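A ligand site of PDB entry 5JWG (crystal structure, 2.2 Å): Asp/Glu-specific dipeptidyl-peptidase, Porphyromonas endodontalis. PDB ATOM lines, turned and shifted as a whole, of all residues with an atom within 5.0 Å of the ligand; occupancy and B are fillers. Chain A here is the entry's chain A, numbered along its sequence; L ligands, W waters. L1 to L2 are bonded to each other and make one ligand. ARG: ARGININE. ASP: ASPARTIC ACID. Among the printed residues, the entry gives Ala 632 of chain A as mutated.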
ATOM      1  N   GLY A  48      -2.086  34.798  26.864  1.00  0.00           N
ATOM      2  CA  GLY A  48      -1.542  33.494  27.208  1.00  0.00           C
ATOM      3  C   GLY A  48      -0.077  33.229  26.849  1.00  0.00           C
ATOM      4  O   GLY A  48       0.341  32.074  26.795  1.00  0.00           O
ATOM      5  N   CYS A  49       0.671  34.287  26.566  1.00  0.00           N
ATOM      6  CA  CYS A  49       2.135  34.228  26.366  1.00  0.00           C
ATOM      7  C   CYS A  49       2.814  35.295  27.205  1.00  0.00           C
ATOM      8  O   CYS A  49       2.171  36.124  27.811  1.00  0.00           O
ATOM      9  CB  CYS A  49       2.565  34.422  24.879  1.00  0.00           C
ATOM     10  SG  CYS A  49       2.567  33.039  23.669  1.00  0.00           S
ATOM     11  N   HIS A  65       5.700  31.667  17.583  1.00  0.00           N
ATOM     12  CA  HIS A  65       4.415  30.990  17.716  1.00  0.00           C
ATOM     13  C   HIS A  65       3.422  31.769  18.616  1.00  0.00           C
ATOM     14  O   HIS A  65       2.222  31.554  18.548  1.00  0.00           O
ATOM     15  CB  HIS A  65       4.608  29.539  18.211  1.00  0.00           C
ATOM     16  CG  HIS A  65       4.810  29.402  19.680  1.00  0.00           C
ATOM     17  ND1 HIS A  65       6.058  29.186  20.231  1.00  0.00           N
ATOM     18  CD2 HIS A  65       3.929  29.395  20.711  1.00  0.00           C
ATOM     19  CE1 HIS A  65       5.934  29.068  21.550  1.00  0.00           C
ATOM     20  NE2 HIS A  65       4.660  29.191  21.865  1.00  0.00           N
ATOM     21  N   LYS A 190       9.519  28.276  12.921  1.00  0.00           N
ATOM     22  CA  LYS A 190       9.058  26.945  13.310  1.00  0.00           C
ATOM     23  C   LYS A 190       9.680  25.847  12.477  1.00  0.00           C
ATOM     24  O   LYS A 190       8.973  24.981  11.958  1.00  0.00           O
ATOM     25  CB  LYS A 190       7.537  26.854  13.253  1.00  0.00           C
ATOM     26  CG  LYS A 190       6.900  27.298  11.977  1.00  0.00           C
ATOM     27  CD  LYS A 190       5.381  27.357  12.127  1.00  0.00           C
ATOM     28  CE  LYS A 190       4.848  26.175  12.909  1.00  0.00           C
ATOM     29  NZ  LYS A 190       3.378  25.989  12.680  1.00  0.00           N
ATOM     30  N   SER A 193       8.545  21.960  12.650  1.00  0.00           N
ATOM     31  CA  SER A 193       7.335  22.309  13.418  1.00  0.00           C
ATOM     32  C   SER A 193       6.633  21.169  14.199  1.00  0.00           C
ATOM     33  O   SER A 193       6.374  21.312  15.379  1.00  0.00           O
ATOM     34  CB  SER A 193       6.305  22.965  12.497  1.00  0.00           C
ATOM     35  OG  SER A 193       5.548  21.995  11.788  1.00  0.00           O
ATOM     36  N   ASN A 197       8.730  19.675  17.639  1.00  0.00           N
ATOM     37  CA  ASN A 197       7.934  20.251  18.733  1.00  0.00           C
ATOM     38  C   ASN A 197       8.013  19.337  19.956  1.00  0.00           C
ATOM     39  O   ASN A 197       8.035  18.109  19.790  1.00  0.00           O
ATOM     40  CB  ASN A 197       6.489  20.440  18.283  1.00  0.00           C
ATOM     41  CG  ASN A 197       5.666  21.285  19.234  1.00  0.00           C
ATOM     42  OD1 ASN A 197       6.192  21.884  20.161  1.00  0.00           O
ATOM     43  ND2 ASN A 197       4.351  21.340  18.998  1.00  0.00           N
ATOM     44  N   TRP A 198       8.110  19.930  21.154  1.00  0.00           N
ATOM     45  CA  TRP A 198       8.340  19.219  22.410  1.00  0.00           C
ATOM     46  C   TRP A 198       9.607  18.356  22.383  1.00  0.00           C
ATOM     47  O   TRP A 198       9.705  17.346  23.094  1.00  0.00           O
ATOM     48  CB  TRP A 198       7.123  18.353  22.789  1.00  0.00           C
ATOM     49  CG  TRP A 198       5.856  19.171  22.903  1.00  0.00           C
ATOM     50  CD1 TRP A 198       4.812  19.217  22.011  1.00  0.00           C
ATOM     51  CD2 TRP A 198       5.528  20.112  23.944  1.00  0.00           C
ATOM     52  NE1 TRP A 198       3.848  20.109  22.446  1.00  0.00           N
ATOM     53  CE2 TRP A 198       4.269  20.668  23.625  1.00  0.00           C
ATOM     54  CE3 TRP A 198       6.179  20.525  25.121  1.00  0.00           C
ATOM     55  CZ2 TRP A 198       3.636  21.614  24.452  1.00  0.00           C
ATOM     56  CZ3 TRP A 198       5.538  21.474  25.937  1.00  0.00           C
ATOM     57  CH2 TRP A 198       4.290  22.004  25.595  1.00  0.00           C
ATOM     58  N   ARG A 202      16.945  21.002  19.691  1.00  0.00           N
ATOM     59  CA  ARG A 202      16.046  21.881  18.962  1.00  0.00           C
ATOM     60  C   ARG A 202      16.888  22.879  18.121  1.00  0.00           C
ATOM     61  O   ARG A 202      18.019  23.196  18.482  1.00  0.00           O
ATOM     62  CB  ARG A 202      15.116  22.603  19.937  1.00  0.00           C
ATOM     63  CG  ARG A 202      13.913  23.287  19.287  1.00  0.00           C
ATOM     64  CD  ARG A 202      12.932  22.294  18.603  1.00  0.00           C
ATOM     65  NE  ARG A 202      11.583  22.855  18.536  1.00  0.00           N
ATOM     66  CZ  ARG A 202      10.722  22.849  19.552  1.00  0.00           C
ATOM     67  NH1 ARG A 202      11.075  22.285  20.715  1.00  0.00           N
ATOM     68  NH2 ARG A 202       9.517  23.382  19.437  1.00  0.00           N
ATOM     69  N   ASP A 206      12.607  30.631  17.141  1.00  0.00           N
ATOM     70  CA  ASP A 206      11.241  30.955  17.539  1.00  0.00           C
ATOM     71  C   ASP A 206      11.099  32.336  18.178  1.00  0.00           C
ATOM     72  O   ASP A 206      11.036  32.449  19.406  1.00  0.00           O
ATOM     73  CB  ASP A 206      10.706  29.858  18.492  1.00  0.00           C
ATOM     74  CG  ASP A 206       9.181  29.902  18.661  1.00  0.00           C
ATOM     75  OD1 ASP A 206       8.564  30.893  18.248  1.00  0.00           O
ATOM     76  OD2 ASP A 206       8.620  28.948  19.230  1.00  0.00           O
ATOM     77  N   ALA A 308      -1.716  24.614  14.040  1.00  0.00           N
ATOM     78  CA  ALA A 308      -0.549  24.681  14.921  1.00  0.00           C
ATOM     79  C   ALA A 308      -0.965  24.543  16.393  1.00  0.00           C
ATOM     80  O   ALA A 308      -0.311  23.871  17.175  1.00  0.00           O
ATOM     81  CB  ALA A 308       0.233  26.005  14.689  1.00  0.00           C
ATOM     82  N   GLN A 311      -2.229  20.759  16.964  1.00  0.00           N
ATOM     83  CA  GLN A 311      -1.077  19.854  17.002  1.00  0.00           C
ATOM     84  C   GLN A 311      -0.279  20.014  18.302  1.00  0.00           C
ATOM     85  O   GLN A 311       0.236  19.034  18.843  1.00  0.00           O
ATOM     86  CB  GLN A 311      -0.157  20.115  15.795  1.00  0.00           C
ATOM     87  CG  GLN A 311       0.959  19.053  15.577  1.00  0.00           C
ATOM     88  CD  GLN A 311       2.195  19.262  16.475  1.00  0.00           C
ATOM     89  OE1 GLN A 311       2.451  20.358  16.969  1.00  0.00           O
ATOM     90  NE2 GLN A 311       2.967  18.198  16.672  1.00  0.00           N
ATOM     91  N   ASN A 312      -0.171  21.245  18.773  1.00  0.00           N
ATOM     92  CA  ASN A 312       0.666  21.536  19.930  1.00  0.00           C
ATOM     93  C   ASN A 312       0.113  20.835  21.168  1.00  0.00           C
ATOM     94  O   ASN A 312       0.873  20.226  21.931  1.00  0.00           O
ATOM     95  CB  ASN A 312       0.787  23.045  20.160  1.00  0.00           C
ATOM     96  CG  ASN A 312       1.743  23.378  21.286  1.00  0.00           C
ATOM     97  OD1 ASN A 312       2.870  22.868  21.321  1.00  0.00           O
ATOM     98  ND2 ASN A 312       1.298  24.209  22.245  1.00  0.00           N
ATOM     99  N   ARG A 316       1.474  17.539  23.174  1.00  0.00           N
ATOM    100  CA  ARG A 316       1.709  17.739  24.595  1.00  0.00           C
ATOM    101  C   ARG A 316       1.021  16.612  25.369  1.00  0.00           C
ATOM    102  O   ARG A 316       1.600  16.045  26.299  1.00  0.00           O
ATOM    103  CB  ARG A 316       1.212  19.110  25.090  1.00  0.00           C
ATOM    104  CG  ARG A 316       1.582  19.382  26.562  1.00  0.00           C
ATOM    105  CD  ARG A 316       1.109  20.746  27.090  1.00  0.00           C
ATOM    106  NE  ARG A 316      -0.346  20.882  26.998  1.00  0.00           N
ATOM    107  CZ  ARG A 316      -0.965  21.810  26.282  1.00  0.00           C
ATOM    108  NH1 ARG A 316      -0.253  22.708  25.601  1.00  0.00           N
ATOM    109  NH2 ARG A 316      -2.295  21.846  26.256  1.00  0.00           N
ATOM    110  N   THR A 627       9.409  25.692  33.682  1.00  0.00           N
ATOM    111  CA  THR A 627       8.440  26.456  32.925  1.00  0.00           C
ATOM    112  C   THR A 627       7.285  25.581  32.471  1.00  0.00           C
ATOM    113  O   THR A 627       7.359  24.362  32.561  1.00  0.00           O
ATOM    114  CB  THR A 627       9.092  27.111  31.687  1.00  0.00           C
ATOM    115  OG1 THR A 627       9.680  26.102  30.861  1.00  0.00           O
ATOM    116  CG2 THR A 627      10.184  28.050  32.130  1.00  0.00           C
ATOM    117  N   THR A 628       6.229  26.215  31.961  1.00  0.00           N
ATOM    118  CA  THR A 628       5.111  25.500  31.329  1.00  0.00           C
ATOM    119  C   THR A 628       4.380  26.438  30.333  1.00  0.00           C
ATOM    120  O   THR A 628       4.759  27.608  30.171  1.00  0.00           O
ATOM    121  CB  THR A 628       4.121  24.958  32.419  1.00  0.00           C
ATOM    122  OG1 THR A 628       3.060  24.190  31.805  1.00  0.00           O
ATOM    123  CG2 THR A 628       3.511  26.098  33.209  1.00  0.00           C
ATOM    124  N   GLY A 629       3.348  25.922  29.655  1.00  0.00           N
ATOM    125  CA  GLY A 629       2.516  26.714  28.770  1.00  0.00           C
ATOM    126  C   GLY A 629       2.194  28.074  29.384  1.00  0.00           C
ATOM    127  O   GLY A 629       1.849  28.155  30.569  1.00  0.00           O
ATOM    128  N   GLY A 630       2.310  29.136  28.592  1.00  0.00           N
ATOM    129  CA  GLY A 630       2.208  30.485  29.141  1.00  0.00           C
ATOM    130  C   GLY A 630       3.586  31.138  29.308  1.00  0.00           C
ATOM    131  O   GLY A 630       3.692  32.379  29.243  1.00  0.00           O
ATOM    132  N   ASN A 631       4.615  30.317  29.532  1.00  0.00           N
ATOM    133  CA  ASN A 631       5.994  30.808  29.618  1.00  0.00           C
ATOM    134  C   ASN A 631       6.665  31.050  28.259  1.00  0.00           C
ATOM    135  O   ASN A 631       7.818  31.494  28.216  1.00  0.00           O
ATOM    136  CB  ASN A 631       6.883  29.848  30.408  1.00  0.00           C
ATOM    137  CG  ASN A 631       6.884  30.118  31.889  1.00  0.00           C
ATOM    138  OD1 ASN A 631       6.660  29.216  32.696  1.00  0.00           O
ATOM    139  ND2 ASN A 631       7.174  31.359  32.257  1.00  0.00           N
ATOM    140  N   ALA A 632       5.975  30.729  27.166  1.00  0.00           N
ATOM    141  CA  ALA A 632       6.503  31.071  25.843  1.00  0.00           C
ATOM    142  C   ALA A 632       6.772  32.576  25.770  1.00  0.00           C
ATOM    143  O   ALA A 632       5.939  33.377  26.188  1.00  0.00           O
ATOM    144  CB  ALA A 632       5.547  30.670  24.738  1.00  0.00           C
ATOM    145  N   ASN A 647      12.625  32.012  26.188  1.00  0.00           N
ATOM    146  CA  ASN A 647      12.082  30.678  26.389  1.00  0.00           C
ATOM    147  C   ASN A 647      10.980  30.361  25.371  1.00  0.00           C
ATOM    148  O   ASN A 647      10.164  31.235  25.067  1.00  0.00           O
ATOM    149  CB  ASN A 647      11.527  30.554  27.813  1.00  0.00           C
ATOM    150  CG  ASN A 647      10.853  29.217  28.063  1.00  0.00           C
ATOM    151  OD1 ASN A 647      11.521  28.190  28.210  1.00  0.00           O
ATOM    152  ND2 ASN A 647       9.535  29.215  28.108  1.00  0.00           N
ATOM    153  N   PHE A 648      10.937  29.133  24.837  1.00  0.00           N
ATOM    154  CA  PHE A 648       9.826  28.836  23.944  1.00  0.00           C
ATOM    155  C   PHE A 648       9.219  27.434  24.017  1.00  0.00           C
ATOM    156  O   PHE A 648       8.130  27.236  23.475  1.00  0.00           O
ATOM    157  CB  PHE A 648      10.195  29.132  22.460  1.00  0.00           C
ATOM    158  CG  PHE A 648      11.255  28.234  21.841  1.00  0.00           C
ATOM    159  CD1 PHE A 648      12.610  28.553  21.944  1.00  0.00           C
ATOM    160  CD2 PHE A 648      10.886  27.155  21.052  1.00  0.00           C
ATOM    161  CE1 PHE A 648      13.573  27.777  21.322  1.00  0.00           C
ATOM    162  CE2 PHE A 648      11.840  26.365  20.416  1.00  0.00           C
ATOM    163  CZ  PHE A 648      13.205  26.677  20.554  1.00  0.00           C
ATOM    164  N   ASP A 649       9.863  26.492  24.703  1.00  0.00           N
ATOM    165  CA  ASP A 649       9.328  25.122  24.775  1.00  0.00           C
ATOM    166  C   ASP A 649       9.912  24.336  25.972  1.00  0.00           C
ATOM    167  O   ASP A 649      10.686  24.872  26.769  1.00  0.00           O
ATOM    168  CB  ASP A 649       9.628  24.361  23.467  1.00  0.00           C
ATOM    169  CG  ASP A 649       8.535  23.343  23.105  1.00  0.00           C
ATOM    170  OD1 ASP A 649       7.634  23.092  23.929  1.00  0.00           O
ATOM    171  OD2 ASP A 649       8.583  22.786  21.996  1.00  0.00           O
ATOM    172  N   ARG A 650       9.491  23.076  26.091  1.00  0.00           N
ATOM    173  CA  ARG A 650      10.116  22.133  27.013  1.00  0.00           C
ATOM    174  C   ARG A 650      10.592  20.892  26.262  1.00  0.00           C
ATOM    175  O   ARG A 650      10.101  20.574  25.167  1.00  0.00           O
ATOM    176  CB  ARG A 650       9.145  21.722  28.117  1.00  0.00           C
ATOM    177  CG  ARG A 650       9.067  22.657  29.321  1.00  0.00           C
ATOM    178  CD  ARG A 650       7.883  22.226  30.204  1.00  0.00           C
ATOM    179  NE  ARG A 650       6.622  22.577  29.559  1.00  0.00           N
ATOM    180  CZ  ARG A 650       5.430  22.093  29.870  1.00  0.00           C
ATOM    181  NH1 ARG A 650       5.321  21.187  30.832  1.00  0.00           N
ATOM    182  NH2 ARG A 650       4.334  22.514  29.219  1.00  0.00           N
HETATM  183  N   ARG L   1       5.406  23.435  22.254  1.00  0.00           N
HETATM  184  CA  ARG L   1       5.581  24.888  22.326  1.00  0.00           C
HETATM  185  C   ARG L   1       4.801  25.393  23.518  1.00  0.00           C
HETATM  186  O   ARG L   1       3.681  24.930  23.755  1.00  0.00           O
HETATM  187  CB  ARG L   1       5.105  25.576  21.031  1.00  0.00           C
HETATM  188  CG  ARG L   1       5.959  25.287  19.798  1.00  0.00           C
HETATM  189  CD  ARG L   1       5.409  25.957  18.551  1.00  0.00           C
HETATM  190  NE  ARG L   1       4.148  25.349  18.107  1.00  0.00           N
HETATM  191  CZ  ARG L   1       4.072  24.348  17.238  1.00  0.00           C
HETATM  192  NH1 ARG L   1       5.172  23.839  16.700  1.00  0.00           N
HETATM  193  NH2 ARG L   1       2.882  23.853  16.900  1.00  0.00           N
HETATM  194  N   ASP L   2       5.377  26.299  24.298  1.00  0.00           N
HETATM  195  CA  ASP L   2       4.673  26.680  25.505  1.00  0.00           C
HETATM  196  C   ASP L   2       3.919  28.001  25.342  1.00  0.00           C
HETATM  197  O   ASP L   2       3.764  28.733  26.327  1.00  0.00           O
HETATM  198  CB  ASP L   2       5.628  26.730  26.695  1.00  0.00           C
HETATM  199  CG  ASP L   2       5.744  25.374  27.398  1.00  0.00           C
HETATM  200  OD1 ASP L   2       4.781  24.572  27.299  1.00  0.00           O
HETATM  201  OD2 ASP L   2       6.765  25.111  28.039  1.00  0.00           O
HETATM  202  OXT ASP L   2       3.447  28.369  24.249  1.00  0.00           O
HETATM  203  O   HOH W   1       1.771  24.424  26.125  1.00  0.00           O
HETATM  204  O   HOH W   2       1.475  26.642  18.831  1.00  0.00           O
HETATM  205  O   HOH W   3       7.700  24.311  16.770  1.00  0.00           O
HETATM  206  O   HOH W   4       9.074  26.310  28.495  1.00  0.00           O
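CH2 of Trp 198 touches OD1 of ASP L2 (3.1 Å). Gln 311 touches the ligand. C of Thr 628 touches CG of ASP L2, at 3.4 Å. N of Asn 631 touches O of ASP L2, 3.7 Å away. Hydrophobic or aromatic side chains within 4 Å of the ligand: His 65, Trp 198 and Ala 632. Of the 23 residues printed, 15 come within 4 Å of the ligand. The nearest printed residue that does not touch the ligand is Arg 202 (4.1 Å).
OD1 of Asn 197 is in hydrogen-bond range of N of ARG L1 (2.7 Å). N of Gly 630 lies within hydrogen-bond range of O of ASP L2 (2.7 Å). OD1 of Asn 312 lies within hydrogen-bond range of N of ARG L1 (2.8 Å). A ring nitrogen (NE2) of His 65 sits at hydrogen-bond distance from an oxygen (OXT) of ASP L2 (2.8 Å). OD1 of Asp 649 lies within salt-bridge range of N of ARG L1, 2.8 Å away. An oxygen (OD1) of ASP L2 is in salt-bridge range of the guanidinium group (NH2) of Arg 650, at 2.8 Å. The backbone carbonyl oxygen (O) of Phe 648 sits at hydrogen-bond distance from a nitrogen (N) of ASP L2, at 3.0 Å. An oxygen (OD1) of ASP L2 lies within hydrogen-bond range of the backbone NH (N) of Gly 629 (3.1 Å). The backbone NH (N) of Ala 632 lies close to an oxygen (O) of ASP L2, 3.1 Å away. A nitrogen (NH1) of ARG L1 sits at hydrogen-bond distance from the backbone carbonyl oxygen (O) of Ser 193, 3.1 Å away. The backbone carbonyl oxygen of Ala 308 is in hydrogen-bond range of a nitrogen (NH2) of ARG L1.
OD1 of Asn 197 sits close to OD2 of Asp 649 (3.1 Å). The backbone carbonyl oxygen (O) of Asn 312 sits at hydrogen-bond distance from the indole nitrogen (NE1) of Trp 198 (3.0 Å). OD2 of Asp 206 is in hydrogen-bond range of ND1 of His 65. The side-chain carboxylate (OD2) of Asp 649 sits at hydrogen-bond distance from the backbone NH (N) of Trp 198 (3.0 Å). NH2 of Arg 202 lies within salt-bridge range of OD2 of Asp 649, at 2.8 Å. The guanidinium group (NH2) of Arg 650 lies within hydrogen-bond range of the side-chain hydroxyl (OG1) of Thr 628, 3.3 Å away. OD1 of Asn 631 is in hydrogen-bond range of N of Thr 628, at 3.1 Å. The backbone carbonyl oxygen (O) of Asn 631 lies within hydrogen-bond range of the side-chain amide nitrogen (ND2) of Asn 647, at 2.9 Å.
Water W3 bridges a nitrogen (NH1) of ARG L1 (2.6 Å) and the guanidinium group (NH2) of Arg 202 (3.4 Å). Water W4 lies within hydrogen-bond range of OG1 of Thr 627, OD2 of ASP L2, O of Asp 649 and ND2 of Asn 647. Water W1 bridges the guanidinium group of Arg 316 (2.7 Å) and an oxygen (O) of ARG L1 (3.1 Å).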
